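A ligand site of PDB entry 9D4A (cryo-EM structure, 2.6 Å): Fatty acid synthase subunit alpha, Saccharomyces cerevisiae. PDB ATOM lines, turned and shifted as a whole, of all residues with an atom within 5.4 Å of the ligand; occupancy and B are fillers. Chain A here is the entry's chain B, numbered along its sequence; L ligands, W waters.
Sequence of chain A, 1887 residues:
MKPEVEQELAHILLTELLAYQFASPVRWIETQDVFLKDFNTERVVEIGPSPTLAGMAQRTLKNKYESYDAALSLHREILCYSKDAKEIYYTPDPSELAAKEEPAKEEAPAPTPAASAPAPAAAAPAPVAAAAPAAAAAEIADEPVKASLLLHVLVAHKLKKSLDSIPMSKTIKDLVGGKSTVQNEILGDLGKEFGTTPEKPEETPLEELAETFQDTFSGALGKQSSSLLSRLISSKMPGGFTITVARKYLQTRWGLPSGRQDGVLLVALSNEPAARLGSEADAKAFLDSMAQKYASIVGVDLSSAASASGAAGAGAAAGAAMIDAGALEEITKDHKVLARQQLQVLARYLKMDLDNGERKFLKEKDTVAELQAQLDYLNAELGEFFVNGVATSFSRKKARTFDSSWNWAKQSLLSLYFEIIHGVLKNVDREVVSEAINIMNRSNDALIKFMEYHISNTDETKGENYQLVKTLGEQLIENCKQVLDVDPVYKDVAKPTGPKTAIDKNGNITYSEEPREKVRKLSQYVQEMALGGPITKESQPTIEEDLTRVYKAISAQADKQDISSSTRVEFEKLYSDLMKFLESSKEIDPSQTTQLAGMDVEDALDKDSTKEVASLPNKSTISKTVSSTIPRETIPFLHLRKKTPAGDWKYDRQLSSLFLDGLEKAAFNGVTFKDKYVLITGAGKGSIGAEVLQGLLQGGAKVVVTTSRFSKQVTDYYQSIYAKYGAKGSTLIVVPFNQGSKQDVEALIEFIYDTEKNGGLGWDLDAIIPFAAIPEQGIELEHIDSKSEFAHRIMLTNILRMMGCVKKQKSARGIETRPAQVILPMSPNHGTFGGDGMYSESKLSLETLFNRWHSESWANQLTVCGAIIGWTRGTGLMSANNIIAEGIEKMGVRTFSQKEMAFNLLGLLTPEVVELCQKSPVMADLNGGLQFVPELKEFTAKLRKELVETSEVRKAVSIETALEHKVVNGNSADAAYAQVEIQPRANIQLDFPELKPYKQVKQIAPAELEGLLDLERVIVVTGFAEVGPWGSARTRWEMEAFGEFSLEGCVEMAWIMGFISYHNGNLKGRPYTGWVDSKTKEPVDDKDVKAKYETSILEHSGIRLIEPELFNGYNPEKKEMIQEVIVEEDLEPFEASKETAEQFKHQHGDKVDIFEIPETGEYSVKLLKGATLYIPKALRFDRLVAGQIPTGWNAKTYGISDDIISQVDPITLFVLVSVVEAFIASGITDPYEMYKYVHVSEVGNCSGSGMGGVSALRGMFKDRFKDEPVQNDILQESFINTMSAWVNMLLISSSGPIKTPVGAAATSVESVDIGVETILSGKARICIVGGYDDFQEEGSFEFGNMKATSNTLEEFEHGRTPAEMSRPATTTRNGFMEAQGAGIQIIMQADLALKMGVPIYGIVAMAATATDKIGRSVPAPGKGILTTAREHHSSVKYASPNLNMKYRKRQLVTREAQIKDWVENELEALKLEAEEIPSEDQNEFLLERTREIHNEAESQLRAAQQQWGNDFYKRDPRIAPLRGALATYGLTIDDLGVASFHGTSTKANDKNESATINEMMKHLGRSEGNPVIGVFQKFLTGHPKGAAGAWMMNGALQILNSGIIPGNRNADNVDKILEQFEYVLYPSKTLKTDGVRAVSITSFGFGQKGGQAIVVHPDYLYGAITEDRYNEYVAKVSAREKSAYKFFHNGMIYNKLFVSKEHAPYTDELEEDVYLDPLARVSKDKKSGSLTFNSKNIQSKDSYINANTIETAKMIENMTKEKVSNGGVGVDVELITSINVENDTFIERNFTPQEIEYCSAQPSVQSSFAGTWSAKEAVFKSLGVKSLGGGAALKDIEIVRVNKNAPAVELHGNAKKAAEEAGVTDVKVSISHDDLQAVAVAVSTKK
O of Arg 520 sits at hydrogen-bond distance from NH2 of Arg 430. NE of Arg 430 is in hydrogen-bond range of O of Val 493, 2.5 Å away. OD1 of Asn 479 lies close to O of Gln 475 (2.8 Å).
Residues that only touch the ligand: Leu 416 (3.5 Å), Ile 420 (3.4 Å), Arg 430 (2.9 Å), Val 433 (3.8 Å), Ala 436 (3.3 Å), Ile 437 (3.9 Å), Met 440 (3.3 Å), Leu 472 (3.8 Å), Gln 475 (3.8 Å), Leu 476 (3.5 Å), Val 493 (3.6 Å) and Lys 521 (3.7 Å). Hydrophobic or aromatic side chains within 4 Å of the ligand: Leu 416, Ile 420, Val 433, Ala 436, Ile 437, Met 440, Leu 472, Leu 476 and Val 493. The nearest printed residue that does not touch the ligand is Val 432 (4.04 Å).
An oxygen (O8) of the ligand sits close to the side-chain amide nitrogen (ND2) of Asn 479 (3.3 Å). The side-chain amino group (NZ) of Lys 491 lies within hydrogen-bond range of an oxygen (O7) of the ligand (3.2 Å). An oxygen (O1) of the ligand is in salt-bridge range of the guanidinium group (NE) of Arg 520, at 3.5 Å.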
ATOM      1  N   LEU A 413     -10.012 -11.975 -21.556  1.00  0.00           N
ATOM      2  CA  LEU A 413     -10.084 -10.706 -20.846  1.00  0.00           C
ATOM      3  C   LEU A 413      -9.157  -9.675 -21.471  1.00  0.00           C
ATOM      4  O   LEU A 413      -9.552  -8.534 -21.694  1.00  0.00           O
ATOM      5  CB  LEU A 413      -9.733 -10.917 -19.371  1.00  0.00           C
ATOM      6  CG  LEU A 413     -10.026  -9.801 -18.363  1.00  0.00           C
ATOM      7  CD1 LEU A 413      -8.965  -8.711 -18.386  1.00  0.00           C
ATOM      8  CD2 LEU A 413     -11.412  -9.186 -18.571  1.00  0.00           C
ATOM      9  N   LEU A 416     -10.631  -8.517 -24.904  1.00  0.00           N
ATOM     10  CA  LEU A 416     -11.742  -7.580 -24.755  1.00  0.00           C
ATOM     11  C   LEU A 416     -11.276  -6.227 -24.244  1.00  0.00           C
ATOM     12  O   LEU A 416     -11.723  -5.176 -24.712  1.00  0.00           O
ATOM     13  CB  LEU A 416     -12.799  -8.166 -23.819  1.00  0.00           C
ATOM     14  CG  LEU A 416     -14.195  -7.543 -23.854  1.00  0.00           C
ATOM     15  CD1 LEU A 416     -14.863  -7.694 -25.219  1.00  0.00           C
ATOM     16  CD2 LEU A 416     -15.052  -8.165 -22.776  1.00  0.00           C
ATOM     17  N   TYR A 417     -10.358  -6.240 -23.277  1.00  0.00           N
ATOM     18  CA  TYR A 417      -9.798  -4.997 -22.748  1.00  0.00           C
ATOM     19  C   TYR A 417      -9.178  -4.175 -23.870  1.00  0.00           C
ATOM     20  O   TYR A 417      -9.521  -2.996 -24.060  1.00  0.00           O
ATOM     21  CB  TYR A 417      -8.768  -5.353 -21.678  1.00  0.00           C
ATOM     22  CG  TYR A 417      -8.059  -4.186 -21.017  1.00  0.00           C
ATOM     23  CD1 TYR A 417      -8.700  -3.408 -20.085  1.00  0.00           C
ATOM     24  CD2 TYR A 417      -6.739  -3.904 -21.309  1.00  0.00           C
ATOM     25  CE1 TYR A 417      -8.062  -2.353 -19.469  1.00  0.00           C
ATOM     26  CE2 TYR A 417      -6.092  -2.852 -20.707  1.00  0.00           C
ATOM     27  CZ  TYR A 417      -6.753  -2.091 -19.784  1.00  0.00           C
ATOM     28  OH  TYR A 417      -6.115  -1.037 -19.168  1.00  0.00           O
ATOM     29  N   ILE A 420     -11.646  -2.734 -26.404  1.00  0.00           N
ATOM     30  CA  ILE A 420     -12.360  -1.566 -25.905  1.00  0.00           C
ATOM     31  C   ILE A 420     -11.464  -0.329 -25.965  1.00  0.00           C
ATOM     32  O   ILE A 420     -11.874   0.714 -26.477  1.00  0.00           O
ATOM     33  CB  ILE A 420     -12.883  -1.814 -24.477  1.00  0.00           C
ATOM     34  CG1 ILE A 420     -13.946  -2.896 -24.485  1.00  0.00           C
ATOM     35  CG2 ILE A 420     -13.464  -0.531 -23.901  1.00  0.00           C
ATOM     36  CD1 ILE A 420     -14.136  -3.567 -23.151  1.00  0.00           C
ATOM     37  N   VAL A 428     -21.180  -0.833 -25.574  1.00  0.00           N
ATOM     38  CA  VAL A 428     -21.443  -2.143 -24.997  1.00  0.00           C
ATOM     39  C   VAL A 428     -22.396  -2.883 -25.924  1.00  0.00           C
ATOM     40  O   VAL A 428     -23.619  -2.818 -25.749  1.00  0.00           O
ATOM     41  CB  VAL A 428     -22.013  -2.040 -23.576  1.00  0.00           C
ATOM     42  CG1 VAL A 428     -22.040  -3.403 -22.907  1.00  0.00           C
ATOM     43  CG2 VAL A 428     -21.223  -1.033 -22.763  1.00  0.00           C
ATOM     44  N   ARG A 430     -23.598  -6.605 -27.959  1.00  0.00           N
ATOM     45  CA  ARG A 430     -23.895  -7.948 -27.461  1.00  0.00           C
ATOM     46  C   ARG A 430     -22.693  -8.867 -27.569  1.00  0.00           C
ATOM     47  O   ARG A 430     -22.591  -9.824 -26.812  1.00  0.00           O
ATOM     48  CB  ARG A 430     -25.101  -8.521 -28.214  1.00  0.00           C
ATOM     49  CG  ARG A 430     -26.345  -7.639 -28.139  1.00  0.00           C
ATOM     50  CD  ARG A 430     -27.026  -7.705 -26.784  1.00  0.00           C
ATOM     51  NE  ARG A 430     -28.109  -8.688 -26.762  1.00  0.00           N
ATOM     52  CZ  ARG A 430     -29.307  -8.501 -27.308  1.00  0.00           C
ATOM     53  NH1 ARG A 430     -29.642  -7.363 -27.895  1.00  0.00           N
ATOM     54  NH2 ARG A 430     -30.207  -9.486 -27.252  1.00  0.00           N
ATOM     55  N   VAL A 432     -19.642  -7.815 -26.801  1.00  0.00           N
ATOM     56  CA  VAL A 432     -18.944  -7.487 -25.562  1.00  0.00           C
ATOM     57  C   VAL A 432     -19.634  -8.155 -24.383  1.00  0.00           C
ATOM     58  O   VAL A 432     -18.971  -8.673 -23.475  1.00  0.00           O
ATOM     59  CB  VAL A 432     -18.872  -5.958 -25.386  1.00  0.00           C
ATOM     60  CG1 VAL A 432     -18.180  -5.599 -24.067  1.00  0.00           C
ATOM     61  CG2 VAL A 432     -18.180  -5.354 -26.560  1.00  0.00           C
ATOM     62  N   VAL A 433     -20.966  -8.150 -24.369  1.00  0.00           N
ATOM     63  CA  VAL A 433     -21.693  -8.819 -23.296  1.00  0.00           C
ATOM     64  C   VAL A 433     -21.406 -10.317 -23.310  1.00  0.00           C
ATOM     65  O   VAL A 433     -21.202 -10.925 -22.250  1.00  0.00           O
ATOM     66  CB  VAL A 433     -23.197  -8.533 -23.398  1.00  0.00           C
ATOM     67  CG1 VAL A 433     -23.951  -9.280 -22.314  1.00  0.00           C
ATOM     68  CG2 VAL A 433     -23.459  -7.044 -23.297  1.00  0.00           C
ATOM     69  N   ALA A 436     -17.931 -10.982 -22.003  1.00  0.00           N
ATOM     70  CA  ALA A 436     -17.969 -10.849 -20.552  1.00  0.00           C
ATOM     71  C   ALA A 436     -18.621 -12.072 -19.915  1.00  0.00           C
ATOM     72  O   ALA A 436     -18.199 -12.517 -18.836  1.00  0.00           O
ATOM     73  CB  ALA A 436     -18.711  -9.583 -20.167  1.00  0.00           C
ATOM     74  N   ILE A 437     -19.659 -12.621 -20.545  1.00  0.00           N
ATOM     75  CA  ILE A 437     -20.317 -13.811 -19.994  1.00  0.00           C
ATOM     76  C   ILE A 437     -19.375 -15.012 -20.027  1.00  0.00           C
ATOM     77  O   ILE A 437     -19.377 -15.839 -19.119  1.00  0.00           O
ATOM     78  CB  ILE A 437     -21.628 -14.097 -20.744  1.00  0.00           C
ATOM     79  CG1 ILE A 437     -22.688 -13.056 -20.388  1.00  0.00           C
ATOM     80  CG2 ILE A 437     -22.144 -15.499 -20.424  1.00  0.00           C
ATOM     81  CD1 ILE A 437     -23.828 -12.973 -21.365  1.00  0.00           C
ATOM     82  N   MET A 440     -16.994 -14.516 -17.185  1.00  0.00           N
ATOM     83  CA  MET A 440     -17.676 -14.881 -15.941  1.00  0.00           C
ATOM     84  C   MET A 440     -17.811 -16.396 -15.805  1.00  0.00           C
ATOM     85  O   MET A 440     -17.677 -16.933 -14.705  1.00  0.00           O
ATOM     86  CB  MET A 440     -19.057 -14.224 -15.883  1.00  0.00           C
ATOM     87  CG  MET A 440     -19.025 -12.712 -15.715  1.00  0.00           C
ATOM     88  SD  MET A 440     -20.509 -11.907 -16.342  1.00  0.00           S
ATOM     89  CE  MET A 440     -21.745 -12.589 -15.253  1.00  0.00           C
ATOM     90  N   ILE A 455      -7.512  -3.491 -14.512  1.00  0.00           N
ATOM     91  CA  ILE A 455      -8.492  -2.402 -14.489  1.00  0.00           C
ATOM     92  C   ILE A 455      -8.104  -1.307 -13.506  1.00  0.00           C
ATOM     93  O   ILE A 455      -8.438  -0.139 -13.716  1.00  0.00           O
ATOM     94  CB  ILE A 455      -9.907  -2.969 -14.196  1.00  0.00           C
ATOM     95  CG1 ILE A 455     -10.310  -4.008 -15.249  1.00  0.00           C
ATOM     96  CG2 ILE A 455     -10.935  -1.842 -14.121  1.00  0.00           C
ATOM     97  CD1 ILE A 455     -10.363  -3.496 -16.680  1.00  0.00           C
ATOM     98  N   VAL A 469     -13.208   1.603 -20.563  1.00  0.00           N
ATOM     99  CA  VAL A 469     -12.714   0.268 -20.246  1.00  0.00           C
ATOM    100  C   VAL A 469     -12.593   0.099 -18.740  1.00  0.00           C
ATOM    101  O   VAL A 469     -12.872  -0.973 -18.198  1.00  0.00           O
ATOM    102  CB  VAL A 469     -11.378  -0.032 -20.965  1.00  0.00           C
ATOM    103  CG1 VAL A 469     -10.160   0.458 -20.194  1.00  0.00           C
ATOM    104  CG2 VAL A 469     -11.234  -1.524 -21.204  1.00  0.00           C
ATOM    105  N   LEU A 472     -16.271  -0.412 -17.380  1.00  0.00           N
ATOM    106  CA  LEU A 472     -16.770  -1.722 -17.753  1.00  0.00           C
ATOM    107  C   LEU A 472     -16.026  -2.822 -17.016  1.00  0.00           C
ATOM    108  O   LEU A 472     -16.626  -3.836 -16.629  1.00  0.00           O
ATOM    109  CB  LEU A 472     -16.635  -1.901 -19.265  1.00  0.00           C
ATOM    110  CG  LEU A 472     -17.674  -1.330 -20.243  1.00  0.00           C
ATOM    111  CD1 LEU A 472     -17.654  -2.135 -21.520  1.00  0.00           C
ATOM    112  CD2 LEU A 472     -19.084  -1.289 -19.675  1.00  0.00           C
ATOM    113  N   GLY A 473     -14.725  -2.637 -16.808  1.00  0.00           N
ATOM    114  CA  GLY A 473     -13.953  -3.640 -16.092  1.00  0.00           C
ATOM    115  C   GLY A 473     -14.307  -3.724 -14.628  1.00  0.00           C
ATOM    116  O   GLY A 473     -14.293  -4.815 -14.048  1.00  0.00           O
ATOM    117  N   GLN A 475     -17.255  -3.086 -13.445  1.00  0.00           N
ATOM    118  CA  GLN A 475     -18.516  -3.812 -13.482  1.00  0.00           C
ATOM    119  C   GLN A 475     -18.290  -5.314 -13.673  1.00  0.00           C
ATOM    120  O   GLN A 475     -18.927  -6.139 -13.006  1.00  0.00           O
ATOM    121  CB  GLN A 475     -19.384  -3.246 -14.606  1.00  0.00           C
ATOM    122  CG  GLN A 475     -20.706  -3.953 -14.817  1.00  0.00           C
ATOM    123  CD  GLN A 475     -21.625  -3.163 -15.733  1.00  0.00           C
ATOM    124  OE1 GLN A 475     -21.226  -2.141 -16.292  1.00  0.00           O
ATOM    125  NE2 GLN A 475     -22.857  -3.635 -15.869  1.00  0.00           N
ATOM    126  N   LEU A 476     -17.363  -5.676 -14.559  1.00  0.00           N
ATOM    127  CA  LEU A 476     -17.071  -7.085 -14.802  1.00  0.00           C
ATOM    128  C   LEU A 476     -16.427  -7.755 -13.586  1.00  0.00           C
ATOM    129  O   LEU A 476     -16.690  -8.927 -13.314  1.00  0.00           O
ATOM    130  CB  LEU A 476     -16.168  -7.224 -16.030  1.00  0.00           C
ATOM    131  CG  LEU A 476     -15.818  -8.646 -16.477  1.00  0.00           C
ATOM    132  CD1 LEU A 476     -17.049  -9.412 -16.876  1.00  0.00           C
ATOM    133  CD2 LEU A 476     -14.833  -8.605 -17.618  1.00  0.00           C
ATOM    134  N   ASN A 479     -19.215  -8.499 -11.305  1.00  0.00           N
ATOM    135  CA  ASN A 479     -20.034  -9.608 -11.777  1.00  0.00           C
ATOM    136  C   ASN A 479     -19.320 -10.944 -11.631  1.00  0.00           C
ATOM    137  O   ASN A 479     -19.959 -11.977 -11.397  1.00  0.00           O
ATOM    138  CB  ASN A 479     -20.454  -9.372 -13.231  1.00  0.00           C
ATOM    139  CG  ASN A 479     -21.268  -8.103 -13.400  1.00  0.00           C
ATOM    140  OD1 ASN A 479     -21.399  -7.303 -12.477  1.00  0.00           O
ATOM    141  ND2 ASN A 479     -21.832  -7.930 -14.586  1.00  0.00           N
ATOM    142  N   LYS A 491     -25.572 -18.808 -21.485  1.00  0.00           N
ATOM    143  CA  LYS A 491     -26.475 -17.699 -21.680  1.00  0.00           C
ATOM    144  C   LYS A 491     -26.165 -17.057 -23.029  1.00  0.00           C
ATOM    145  O   LYS A 491     -25.064 -16.536 -23.222  1.00  0.00           O
ATOM    146  CB  LYS A 491     -26.358 -16.682 -20.550  1.00  0.00           C
ATOM    147  CG  LYS A 491     -27.439 -15.620 -20.537  1.00  0.00           C
ATOM    148  CD  LYS A 491     -27.352 -14.746 -19.295  1.00  0.00           C
ATOM    149  CE  LYS A 491     -28.358 -13.618 -19.351  1.00  0.00           C
ATOM    150  NZ  LYS A 491     -28.368 -12.829 -18.085  1.00  0.00           N
ATOM    151  N   VAL A 493     -26.748 -14.182 -25.755  1.00  0.00           N
ATOM    152  CA  VAL A 493     -27.124 -12.783 -25.752  1.00  0.00           C
ATOM    153  C   VAL A 493     -27.065 -12.146 -27.122  1.00  0.00           C
ATOM    154  O   VAL A 493     -27.244 -10.933 -27.241  1.00  0.00           O
ATOM    155  CB  VAL A 493     -26.249 -11.975 -24.763  1.00  0.00           C
ATOM    156  CG1 VAL A 493     -26.590 -12.355 -23.338  1.00  0.00           C
ATOM    157  CG2 VAL A 493     -24.768 -12.205 -25.040  1.00  0.00           C
ATOM    158  N   ARG A 520     -35.955  -9.063 -29.643  1.00  0.00           N
ATOM    159  CA  ARG A 520     -34.642  -8.467 -29.444  1.00  0.00           C
ATOM    160  C   ARG A 520     -33.777  -9.232 -28.436  1.00  0.00           C
ATOM    161  O   ARG A 520     -32.558  -9.017 -28.418  1.00  0.00           O
ATOM    162  CB  ARG A 520     -34.804  -6.991 -29.012  1.00  0.00           C
ATOM    163  CG  ARG A 520     -33.732  -6.328 -28.118  1.00  0.00           C
ATOM    164  CD  ARG A 520     -34.305  -5.099 -27.423  1.00  0.00           C
ATOM    165  NE  ARG A 520     -34.863  -5.407 -26.103  1.00  0.00           N
ATOM    166  CZ  ARG A 520     -35.873  -4.773 -25.525  1.00  0.00           C
ATOM    167  NH1 ARG A 520     -36.538  -3.811 -26.143  1.00  0.00           N
ATOM    168  NH2 ARG A 520     -36.225  -5.106 -24.283  1.00  0.00           N
ATOM    169  N   LYS A 521     -34.365 -10.104 -27.624  1.00  0.00           N
ATOM    170  CA  LYS A 521     -33.642 -10.883 -26.628  1.00  0.00           C
ATOM    171  C   LYS A 521     -34.072 -12.338 -26.742  1.00  0.00           C
ATOM    172  O   LYS A 521     -35.086 -12.656 -27.380  1.00  0.00           O
ATOM    173  CB  LYS A 521     -33.919 -10.367 -25.210  1.00  0.00           C
ATOM    174  CG  LYS A 521     -33.294  -9.017 -24.903  1.00  0.00           C
ATOM    175  CD  LYS A 521     -34.089  -8.248 -23.858  1.00  0.00           C
ATOM    176  CE  LYS A 521     -34.047  -8.919 -22.493  1.00  0.00           C
ATOM    177  NZ  LYS A 521     -34.732  -8.118 -21.447  1.00  0.00           N
HETATM  178  O1  LIG L   1     -31.779  -4.820 -24.565  1.00  0.00           O
HETATM  179  P1  LIG L   1     -30.701  -5.023 -23.327  1.00  0.00           P
HETATM  180  O2  LIG L   1     -31.253  -4.588 -22.014  1.00  0.00           O
HETATM  181  O3  LIG L   1     -29.453  -4.288 -23.690  1.00  0.00           O
HETATM  182  O4  LIG L   1     -30.435  -6.637 -23.235  1.00  0.00           O
HETATM  183  C1  LIG L   1     -29.759  -7.346 -24.221  1.00  0.00           C
HETATM  184  C2  LIG L   1     -29.112  -8.474 -23.458  1.00  0.00           C
HETATM  185  C3  LIG L   1     -29.920  -9.739 -23.614  1.00  0.00           C
HETATM  186  C4  LIG L   1     -27.699  -8.757 -23.873  1.00  0.00           C
HETATM  187  C5  LIG L   1     -28.978  -8.002 -22.038  1.00  0.00           C
HETATM  188  O5  LIG L   1     -27.670  -7.603 -21.811  1.00  0.00           O
HETATM  189  C6  LIG L   1     -29.484  -9.013 -21.071  1.00  0.00           C
HETATM  190  O6  LIG L   1     -30.647  -9.013 -20.906  1.00  0.00           O
HETATM  191  N1  LIG L   1     -28.674  -9.974 -20.366  1.00  0.00           N
HETATM  192  C7  LIG L   1     -27.247 -10.065 -20.490  1.00  0.00           C
HETATM  193  C8  LIG L   1     -26.711  -9.143 -19.427  1.00  0.00           C
HETATM  194  C9  LIG L   1     -25.651  -9.899 -18.678  1.00  0.00           C
HETATM  195  O7  LIG L   1     -25.715 -11.045 -18.582  1.00  0.00           O
HETATM  196  N2  LIG L   1     -24.557  -9.242 -18.089  1.00  0.00           N
HETATM  197  C10 LIG L   1     -23.651 -10.107 -17.425  1.00  0.00           C
HETATM  198  C11 LIG L   1     -22.412  -9.344 -17.076  1.00  0.00           C
HETATM  199  S1  LIG L   1     -21.546  -8.874 -18.564  1.00  0.00           S
HETATM  200  C12 LIG L   1     -20.733  -7.247 -18.377  1.00  0.00           C
HETATM  201  O8  LIG L   1     -20.430  -6.830 -17.338  1.00  0.00           O
HETATM  202  C13 LIG L   1     -20.438  -6.385 -19.569  1.00  0.00           C
HETATM  203  C14 LIG L   1     -19.147  -5.574 -19.516  1.00  0.00           C
HETATM  204  C15 LIG L   1     -17.808  -6.303 -19.462  1.00  0.00           C
HETATM  205  C16 LIG L   1     -16.696  -5.704 -20.309  1.00  0.00           C
HETATM  206  C17 LIG L   1     -15.361  -5.825 -19.610  1.00  0.00           C
HETATM  207  C18 LIG L   1     -14.101  -5.740 -20.479  1.00  0.00           C
HETATM  208  C19 LIG L   1     -12.824  -5.123 -19.870  1.00  0.00           C
HETATM  209  O   HOH W   1     -32.331  -2.763 -20.514  1.00  0.00           O
HETATM  210  O   HOH W   2     -28.457  -3.905 -25.912  1.00  0.00           O
